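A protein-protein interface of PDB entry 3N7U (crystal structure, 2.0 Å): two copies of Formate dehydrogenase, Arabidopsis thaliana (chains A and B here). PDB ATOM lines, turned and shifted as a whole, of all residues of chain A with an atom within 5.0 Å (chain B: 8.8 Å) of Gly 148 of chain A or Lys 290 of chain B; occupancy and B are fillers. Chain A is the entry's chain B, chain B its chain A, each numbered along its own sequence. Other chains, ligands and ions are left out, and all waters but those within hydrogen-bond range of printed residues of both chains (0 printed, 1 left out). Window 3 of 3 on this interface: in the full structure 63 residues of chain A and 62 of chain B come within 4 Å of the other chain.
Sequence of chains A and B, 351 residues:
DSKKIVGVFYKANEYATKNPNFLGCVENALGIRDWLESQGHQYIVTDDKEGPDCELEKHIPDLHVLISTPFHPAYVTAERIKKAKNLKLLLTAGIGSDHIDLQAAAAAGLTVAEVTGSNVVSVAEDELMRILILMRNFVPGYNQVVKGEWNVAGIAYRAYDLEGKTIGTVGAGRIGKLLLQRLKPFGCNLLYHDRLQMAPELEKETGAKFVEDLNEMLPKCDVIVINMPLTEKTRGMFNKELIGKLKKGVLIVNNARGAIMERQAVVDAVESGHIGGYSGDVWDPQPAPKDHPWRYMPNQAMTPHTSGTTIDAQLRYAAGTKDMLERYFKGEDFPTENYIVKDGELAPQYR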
ATOM      1  N   GLN A 144     -12.294 -13.521  13.888  1.00  0.00           N
ATOM      2  CA  GLN A 144     -12.856 -12.657  14.914  1.00  0.00           C
ATOM      3  C   GLN A 144     -13.424 -13.516  16.054  1.00  0.00           C
ATOM      4  O   GLN A 144     -13.224 -13.193  17.243  1.00  0.00           O
ATOM      5  CB  GLN A 144     -14.017 -11.785  14.332  1.00  0.00           C
ATOM      6  CG  GLN A 144     -13.616 -10.535  13.512  1.00  0.00           C
ATOM      7  CD  GLN A 144     -14.814  -9.646  13.140  1.00  0.00           C
ATOM      8  OE1 GLN A 144     -15.873  -9.715  13.786  1.00  0.00           O
ATOM      9  NE2 GLN A 144     -14.658  -8.823  12.087  1.00  0.00           N
ATOM     10  N   VAL A 145     -14.170 -14.582  15.693  1.00  0.00           N
ATOM     11  CA  VAL A 145     -14.762 -15.472  16.704  1.00  0.00           C
ATOM     12  C   VAL A 145     -13.698 -15.984  17.675  1.00  0.00           C
ATOM     13  O   VAL A 145     -13.861 -15.843  18.909  1.00  0.00           O
ATOM     14  CB  VAL A 145     -15.549 -16.654  16.052  1.00  0.00           C
ATOM     15  CG1 VAL A 145     -15.729 -17.842  17.001  1.00  0.00           C
ATOM     16  CG2 VAL A 145     -16.868 -16.154  15.585  1.00  0.00           C
ATOM     17  N   VAL A 146     -12.602 -16.563  17.149  1.00  0.00           N
ATOM     18  CA  VAL A 146     -11.605 -17.197  18.049  1.00  0.00           C
ATOM     19  C   VAL A 146     -10.767 -16.172  18.868  1.00  0.00           C
ATOM     20  O   VAL A 146     -10.259 -16.522  19.963  1.00  0.00           O
ATOM     21  CB  VAL A 146     -10.696 -18.290  17.351  1.00  0.00           C
ATOM     22  CG1 VAL A 146     -11.545 -19.397  16.681  1.00  0.00           C
ATOM     23  CG2 VAL A 146      -9.750 -17.661  16.319  1.00  0.00           C
ATOM     24  N   LYS A 147     -10.621 -14.943  18.342  1.00  0.00           N
ATOM     25  CA  LYS A 147      -9.897 -13.860  19.036  1.00  0.00           C
ATOM     26  C   LYS A 147     -10.800 -13.077  19.970  1.00  0.00           C
ATOM     27  O   LYS A 147     -10.345 -12.170  20.649  1.00  0.00           O
ATOM     28  CB  LYS A 147      -9.261 -12.869  18.059  1.00  0.00           C
ATOM     29  CG  LYS A 147      -8.159 -13.431  17.236  1.00  0.00           C
ATOM     30  CD  LYS A 147      -7.782 -12.409  16.179  1.00  0.00           C
ATOM     31  CE  LYS A 147      -6.785 -12.950  15.182  1.00  0.00           C
ATOM     32  NZ  LYS A 147      -6.444 -11.802  14.292  1.00  0.00           N
ATOM     33  N   GLY A 148     -12.079 -13.450  20.045  1.00  0.00           N
ATOM     34  CA  GLY A 148     -12.991 -12.776  20.971  1.00  0.00           C
ATOM     35  C   GLY A 148     -13.514 -11.424  20.488  1.00  0.00           C
ATOM     36  O   GLY A 148     -14.055 -10.638  21.295  1.00  0.00           O
ATOM     37  N   GLU A 149     -13.384 -11.162  19.183  1.00  0.00           N
ATOM     38  CA  GLU A 149     -13.835  -9.916  18.591  1.00  0.00           C
ATOM     39  C   GLU A 149     -15.276  -9.968  18.050  1.00  0.00           C
ATOM     40  O   GLU A 149     -15.866 -11.072  17.867  1.00  0.00           O
ATOM     41  CB  GLU A 149     -12.877  -9.535  17.463  1.00  0.00           C
ATOM     42  CG  GLU A 149     -11.447  -9.397  17.948  1.00  0.00           C
ATOM     43  CD  GLU A 149     -10.454  -9.179  16.818  1.00  0.00           C
ATOM     44  OE1 GLU A 149     -10.767  -9.489  15.665  1.00  0.00           O
ATOM     45  OE2 GLU A 149      -9.322  -8.769  17.100  1.00  0.00           O
ATOM     46  N   TRP A 150     -15.839  -8.786  17.774  1.00  0.00           N
ATOM     47  CA  TRP A 150     -17.133  -8.688  17.080  1.00  0.00           C
ATOM     48  C   TRP A 150     -17.216  -7.408  16.259  1.00  0.00           C
ATOM     49  O   TRP A 150     -17.379  -6.323  16.834  1.00  0.00           O
ATOM     50  CB  TRP A 150     -18.330  -8.790  18.063  1.00  0.00           C
ATOM     51  CG  TRP A 150     -19.687  -8.768  17.349  1.00  0.00           C
ATOM     52  CD1 TRP A 150     -20.324  -7.658  16.784  1.00  0.00           C
ATOM     53  CD2 TRP A 150     -20.553  -9.883  17.110  1.00  0.00           C
ATOM     54  NE1 TRP A 150     -21.530  -8.034  16.225  1.00  0.00           N
ATOM     55  CE2 TRP A 150     -21.700  -9.386  16.410  1.00  0.00           C
ATOM     56  CE3 TRP A 150     -20.495 -11.266  17.441  1.00  0.00           C
ATOM     57  CZ2 TRP A 150     -22.788 -10.228  16.031  1.00  0.00           C
ATOM     58  CZ3 TRP A 150     -21.575 -12.098  17.062  1.00  0.00           C
ATOM     59  CH2 TRP A 150     -22.702 -11.571  16.358  1.00  0.00           C
ATOM     60  N   TRP B 283     -26.424 -15.654  17.111  1.00  0.00           N
ATOM     61  CA  TRP B 283     -26.048 -15.842  18.527  1.00  0.00           C
ATOM     62  C   TRP B 283     -27.086 -15.233  19.418  1.00  0.00           C
ATOM     63  O   TRP B 283     -27.848 -14.383  18.967  1.00  0.00           O
ATOM     64  CB  TRP B 283     -24.736 -15.117  18.842  1.00  0.00           C
ATOM     65  CG  TRP B 283     -23.553 -15.405  17.909  1.00  0.00           C
ATOM     66  CD1 TRP B 283     -23.434 -15.087  16.573  1.00  0.00           C
ATOM     67  CD2 TRP B 283     -22.318 -16.018  18.281  1.00  0.00           C
ATOM     68  NE1 TRP B 283     -22.205 -15.500  16.102  1.00  0.00           N
ATOM     69  CE2 TRP B 283     -21.498 -16.053  17.135  1.00  0.00           C
ATOM     70  CE3 TRP B 283     -21.823 -16.548  19.489  1.00  0.00           C
ATOM     71  CZ2 TRP B 283     -20.233 -16.597  17.147  1.00  0.00           C
ATOM     72  CZ3 TRP B 283     -20.516 -17.071  19.503  1.00  0.00           C
ATOM     73  CH2 TRP B 283     -19.743 -17.090  18.344  1.00  0.00           C
ATOM     74  N   PRO B 285     -26.845 -13.211  23.120  1.00  0.00           N
ATOM     75  CA  PRO B 285     -27.368 -12.041  22.410  1.00  0.00           C
ATOM     76  C   PRO B 285     -26.397 -11.619  21.310  1.00  0.00           C
ATOM     77  O   PRO B 285     -25.343 -12.256  21.146  1.00  0.00           O
ATOM     78  CB  PRO B 285     -27.402 -10.961  23.515  1.00  0.00           C
ATOM     79  CG  PRO B 285     -26.185 -11.288  24.379  1.00  0.00           C
ATOM     80  CD  PRO B 285     -26.009 -12.819  24.276  1.00  0.00           C
ATOM     81  N   PRO B 287     -24.428  -7.908  19.903  1.00  0.00           N
ATOM     82  CA  PRO B 287     -23.125  -8.586  19.711  1.00  0.00           C
ATOM     83  C   PRO B 287     -22.897  -9.680  20.734  1.00  0.00           C
ATOM     84  O   PRO B 287     -23.292  -9.526  21.899  1.00  0.00           O
ATOM     85  CB  PRO B 287     -22.093  -7.452  19.914  1.00  0.00           C
ATOM     86  CG  PRO B 287     -22.859  -6.174  19.420  1.00  0.00           C
ATOM     87  CD  PRO B 287     -24.252  -6.436  20.041  1.00  0.00           C
ATOM     88  N   ALA B 288     -22.257 -10.773  20.311  1.00  0.00           N
ATOM     89  CA  ALA B 288     -21.871 -11.833  21.240  1.00  0.00           C
ATOM     90  C   ALA B 288     -20.721 -11.360  22.134  1.00  0.00           C
ATOM     91  O   ALA B 288     -19.715 -10.884  21.635  1.00  0.00           O
ATOM     92  CB  ALA B 288     -21.471 -13.097  20.471  1.00  0.00           C
ATOM     93  N   PRO B 289     -20.888 -11.457  23.474  1.00  0.00           N
ATOM     94  CA  PRO B 289     -19.787 -11.057  24.337  1.00  0.00           C
ATOM     95  C   PRO B 289     -18.491 -11.857  24.053  1.00  0.00           C
ATOM     96  O   PRO B 289     -18.519 -12.966  23.485  1.00  0.00           O
ATOM     97  CB  PRO B 289     -20.319 -11.340  25.766  1.00  0.00           C
ATOM     98  CG  PRO B 289     -21.821 -11.274  25.649  1.00  0.00           C
ATOM     99  CD  PRO B 289     -22.108 -11.809  24.242  1.00  0.00           C
ATOM    100  N   LYS B 290     -17.379 -11.279  24.455  1.00  0.00           N
ATOM    101  CA  LYS B 290     -16.080 -11.894  24.350  1.00  0.00           C
ATOM    102  C   LYS B 290     -16.007 -13.277  24.975  1.00  0.00           C
ATOM    103  O   LYS B 290     -15.286 -14.121  24.467  1.00  0.00           O
ATOM    104  CB  LYS B 290     -15.067 -10.988  25.038  1.00  0.00           C
ATOM    105  CG  LYS B 290     -13.625 -11.403  24.855  1.00  0.00           C
ATOM    106  CD  LYS B 290     -12.714 -10.403  25.599  1.00  0.00           C
ATOM    107  CE  LYS B 290     -11.429 -11.058  26.105  1.00  0.00           C
ATOM    108  NZ  LYS B 290     -10.675 -11.807  25.030  1.00  0.00           N
ATOM    109  N   ASP B 291     -16.716 -13.504  26.085  1.00  0.00           N
ATOM    110  CA  ASP B 291     -16.678 -14.817  26.746  1.00  0.00           C
ATOM    111  C   ASP B 291     -17.745 -15.828  26.268  1.00  0.00           C
ATOM    112  O   ASP B 291     -17.878 -16.878  26.874  1.00  0.00           O
ATOM    113  CB  ASP B 291     -16.714 -14.686  28.295  1.00  0.00           C
ATOM    114  CG  ASP B 291     -18.043 -14.117  28.847  1.00  0.00           C
ATOM    115  OD1 ASP B 291     -18.994 -13.796  28.073  1.00  0.00           O
ATOM    116  OD2 ASP B 291     -18.125 -13.972  30.104  1.00  0.00           O
ATOM    117  N   HIS B 292     -18.508 -15.514  25.214  1.00  0.00           N
ATOM    118  CA  HIS B 292     -19.599 -16.414  24.786  1.00  0.00           C
ATOM    119  C   HIS B 292     -18.998 -17.790  24.445  1.00  0.00           C
ATOM    120  O   HIS B 292     -18.056 -17.863  23.647  1.00  0.00           O
ATOM    121  CB  HIS B 292     -20.370 -15.866  23.587  1.00  0.00           C
ATOM    122  CG  HIS B 292     -21.636 -16.622  23.283  1.00  0.00           C
ATOM    123  ND1 HIS B 292     -21.658 -17.944  22.891  1.00  0.00           N
ATOM    124  CD2 HIS B 292     -22.923 -16.213  23.279  1.00  0.00           C
ATOM    125  CE1 HIS B 292     -22.903 -18.321  22.674  1.00  0.00           C
ATOM    126  NE2 HIS B 292     -23.689 -17.283  22.895  1.00  0.00           N
ATOM    127  N   PRO B 293     -19.502 -18.875  25.088  1.00  0.00           N
ATOM    128  CA  PRO B 293     -18.784 -20.163  25.020  1.00  0.00           C
ATOM    129  C   PRO B 293     -18.824 -20.874  23.660  1.00  0.00           C
ATOM    130  O   PRO B 293     -18.020 -21.780  23.455  1.00  0.00           O
ATOM    131  CB  PRO B 293     -19.497 -21.028  26.085  1.00  0.00           C
ATOM    132  CG  PRO B 293     -20.922 -20.477  26.065  1.00  0.00           C
ATOM    133  CD  PRO B 293     -20.713 -18.964  25.925  1.00  0.00           C
ATOM    134  N   TRP B 294     -19.747 -20.504  22.766  1.00  0.00           N
ATOM    135  CA  TRP B 294     -19.767 -21.063  21.391  1.00  0.00           C
ATOM    136  C   TRP B 294     -18.483 -20.709  20.606  1.00  0.00           C
ATOM    137  O   TRP B 294     -18.098 -21.412  19.631  1.00  0.00           O
ATOM    138  CB  TRP B 294     -21.015 -20.613  20.623  1.00  0.00           C
ATOM    139  CG  TRP B 294     -22.306 -21.311  21.029  1.00  0.00           C
ATOM    140  CD1 TRP B 294     -22.470 -22.213  22.063  1.00  0.00           C
ATOM    141  CD2 TRP B 294     -23.606 -21.098  20.482  1.00  0.00           C
ATOM    142  NE1 TRP B 294     -23.786 -22.614  22.137  1.00  0.00           N
ATOM    143  CE2 TRP B 294     -24.509 -21.934  21.195  1.00  0.00           C
ATOM    144  CE3 TRP B 294     -24.112 -20.287  19.430  1.00  0.00           C
ATOM    145  CZ2 TRP B 294     -25.891 -22.008  20.879  1.00  0.00           C
ATOM    146  CZ3 TRP B 294     -25.470 -20.351  19.134  1.00  0.00           C
ATOM    147  CH2 TRP B 294     -26.344 -21.203  19.860  1.00  0.00           C
ATOM    148  N   ARG B 295     -17.793 -19.659  21.060  1.00  0.00           N
ATOM    149  CA  ARG B 295     -16.578 -19.200  20.397  1.00  0.00           C
ATOM    150  C   ARG B 295     -15.446 -20.185  20.624  1.00  0.00           C
ATOM    151  O   ARG B 295     -14.530 -20.250  19.817  1.00  0.00           O
ATOM    152  CB  ARG B 295     -16.101 -17.840  20.942  1.00  0.00           C
ATOM    153  CG  ARG B 295     -16.966 -16.625  20.721  1.00  0.00           C
ATOM    154  CD  ARG B 295     -16.380 -15.463  21.584  1.00  0.00           C
ATOM    155  NE  ARG B 295     -17.051 -14.176  21.319  1.00  0.00           N
ATOM    156  CZ  ARG B 295     -16.717 -13.357  20.334  1.00  0.00           C
ATOM    157  NH1 ARG B 295     -15.728 -13.683  19.499  1.00  0.00           N
ATOM    158  NH2 ARG B 295     -17.382 -12.223  20.161  1.00  0.00           N
ATOM    159  N   TYR B 296     -15.512 -20.956  21.717  1.00  0.00           N
ATOM    160  CA  TYR B 296     -14.342 -21.732  22.203  1.00  0.00           C
ATOM    161  C   TYR B 296     -14.503 -23.254  22.237  1.00  0.00           C
ATOM    162  O   TYR B 296     -13.525 -23.964  22.438  1.00  0.00           O
ATOM    163  CB  TYR B 296     -13.856 -21.186  23.583  1.00  0.00           C
ATOM    164  CG  TYR B 296     -13.662 -19.672  23.559  1.00  0.00           C
ATOM    165  CD1 TYR B 296     -14.504 -18.818  24.285  1.00  0.00           C
ATOM    166  CD2 TYR B 296     -12.696 -19.095  22.719  1.00  0.00           C
ATOM    167  CE1 TYR B 296     -14.347 -17.426  24.221  1.00  0.00           C
ATOM    168  CE2 TYR B 296     -12.525 -17.731  22.661  1.00  0.00           C
ATOM    169  CZ  TYR B 296     -13.357 -16.899  23.400  1.00  0.00           C
ATOM    170  OH  TYR B 296     -13.178 -15.539  23.294  1.00  0.00           O
ATOM    171  N   PRO B 304     -19.419 -14.036  13.143  1.00  0.00           N
ATOM    172  CA  PRO B 304     -20.494 -13.118  13.559  1.00  0.00           C
ATOM    173  C   PRO B 304     -21.624 -13.114  12.540  1.00  0.00           C
ATOM    174  O   PRO B 304     -21.530 -13.808  11.513  1.00  0.00           O
ATOM    175  CB  PRO B 304     -19.793 -11.739  13.580  1.00  0.00           C
ATOM    176  CG  PRO B 304     -18.264 -12.075  13.790  1.00  0.00           C
ATOM    177  CD  PRO B 304     -18.176 -13.293  12.818  1.00  0.00           C
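Among the printed residues, pairs that only touch across the chains: Gln 144 of chain A with Pro 304 of chain B, Val 145 of chain A with Trp 283 of chain B, Val 146 of chain A with Tyr 296 of chain B, Gly 148 of chain A with Lys 290 of chain B, Gly 148 of chain A with Arg 295 of chain B, Gly 148 of chain A with Tyr 296 of chain B, Trp 150 of chain A with Trp 283 of chain B, Trp 150 of chain A with Pro 287 of chain B, Trp 150 of chain A with Ala 288 of chain B and Trp 150 of chain A with Pro 304 of chain B.
No position is printed for both chains.
Of the 13 pairs that touch across the chains among the printed residues, none has its exchanged pair printed and touching as well.
Of the 13 printed residues of chain B, 7 touch a printed residue of chain A.
Hydrophobic or aromatic side chains of chain B within 4 Å of the printed part of chain A: Trp 283, Pro 287, Ala 288, Tyr 296 and Pro 304.
Along chain B the printed residues that touch a printed residue of chain A span positions 283 to 304.
Among the printed residues, 13 pairs touch across the chains.
NH2 of Arg 295 of chain B lies within hydrogen-bond range of O of Glu 149 of chain A (3.0 Å).
NH1 of Arg 295 of chain B sits at hydrogen-bond distance from O of Gln 144 of chain A (3.4 Å).
NH1 of Arg 295 of chain B lies within hydrogen-bond range of O of Val 145 of chain A (2.9 Å).
Of the printed residues of chain B, Val 146 of chain A touches Tyr 296 (3.7 Å).
Printed residues of chain B within 4 Å of Trp 150 of chain A: Trp 283, Pro 287, Ala 288 and Pro 304.
Of the printed residues of chain A, Trp 283 of chain B touches Val 145 (3.7 Å) and Trp 150 (3.6 Å).
Printed residues of chain A within 4 Å of Pro 304 of chain B: Gln 144 (3.4 Å) and Trp 150 (3.8 Å).
The nearest printed residue of chain B that does not touch Val 145 of chain A is Pro 304 of chain B (4.1 Å).
The backbone carbonyl oxygen (O) of Pro 289 of chain B is in hydrogen-bond range of the guanidinium group (NE) of Arg 295 of chain B (2.9 Å).
O of Ala 288 of chain B is in hydrogen-bond range of NH2 of Arg 295 of chain B.
The backbone carbonyl oxygen of Gln 144 of chain A lies within hydrogen-bond range of the backbone NH of Glu 149 of chain A (2.8 Å).
OH of Tyr 296 of chain B sits at hydrogen-bond distance from O of Lys 290 of chain B, 2.8 Å away.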
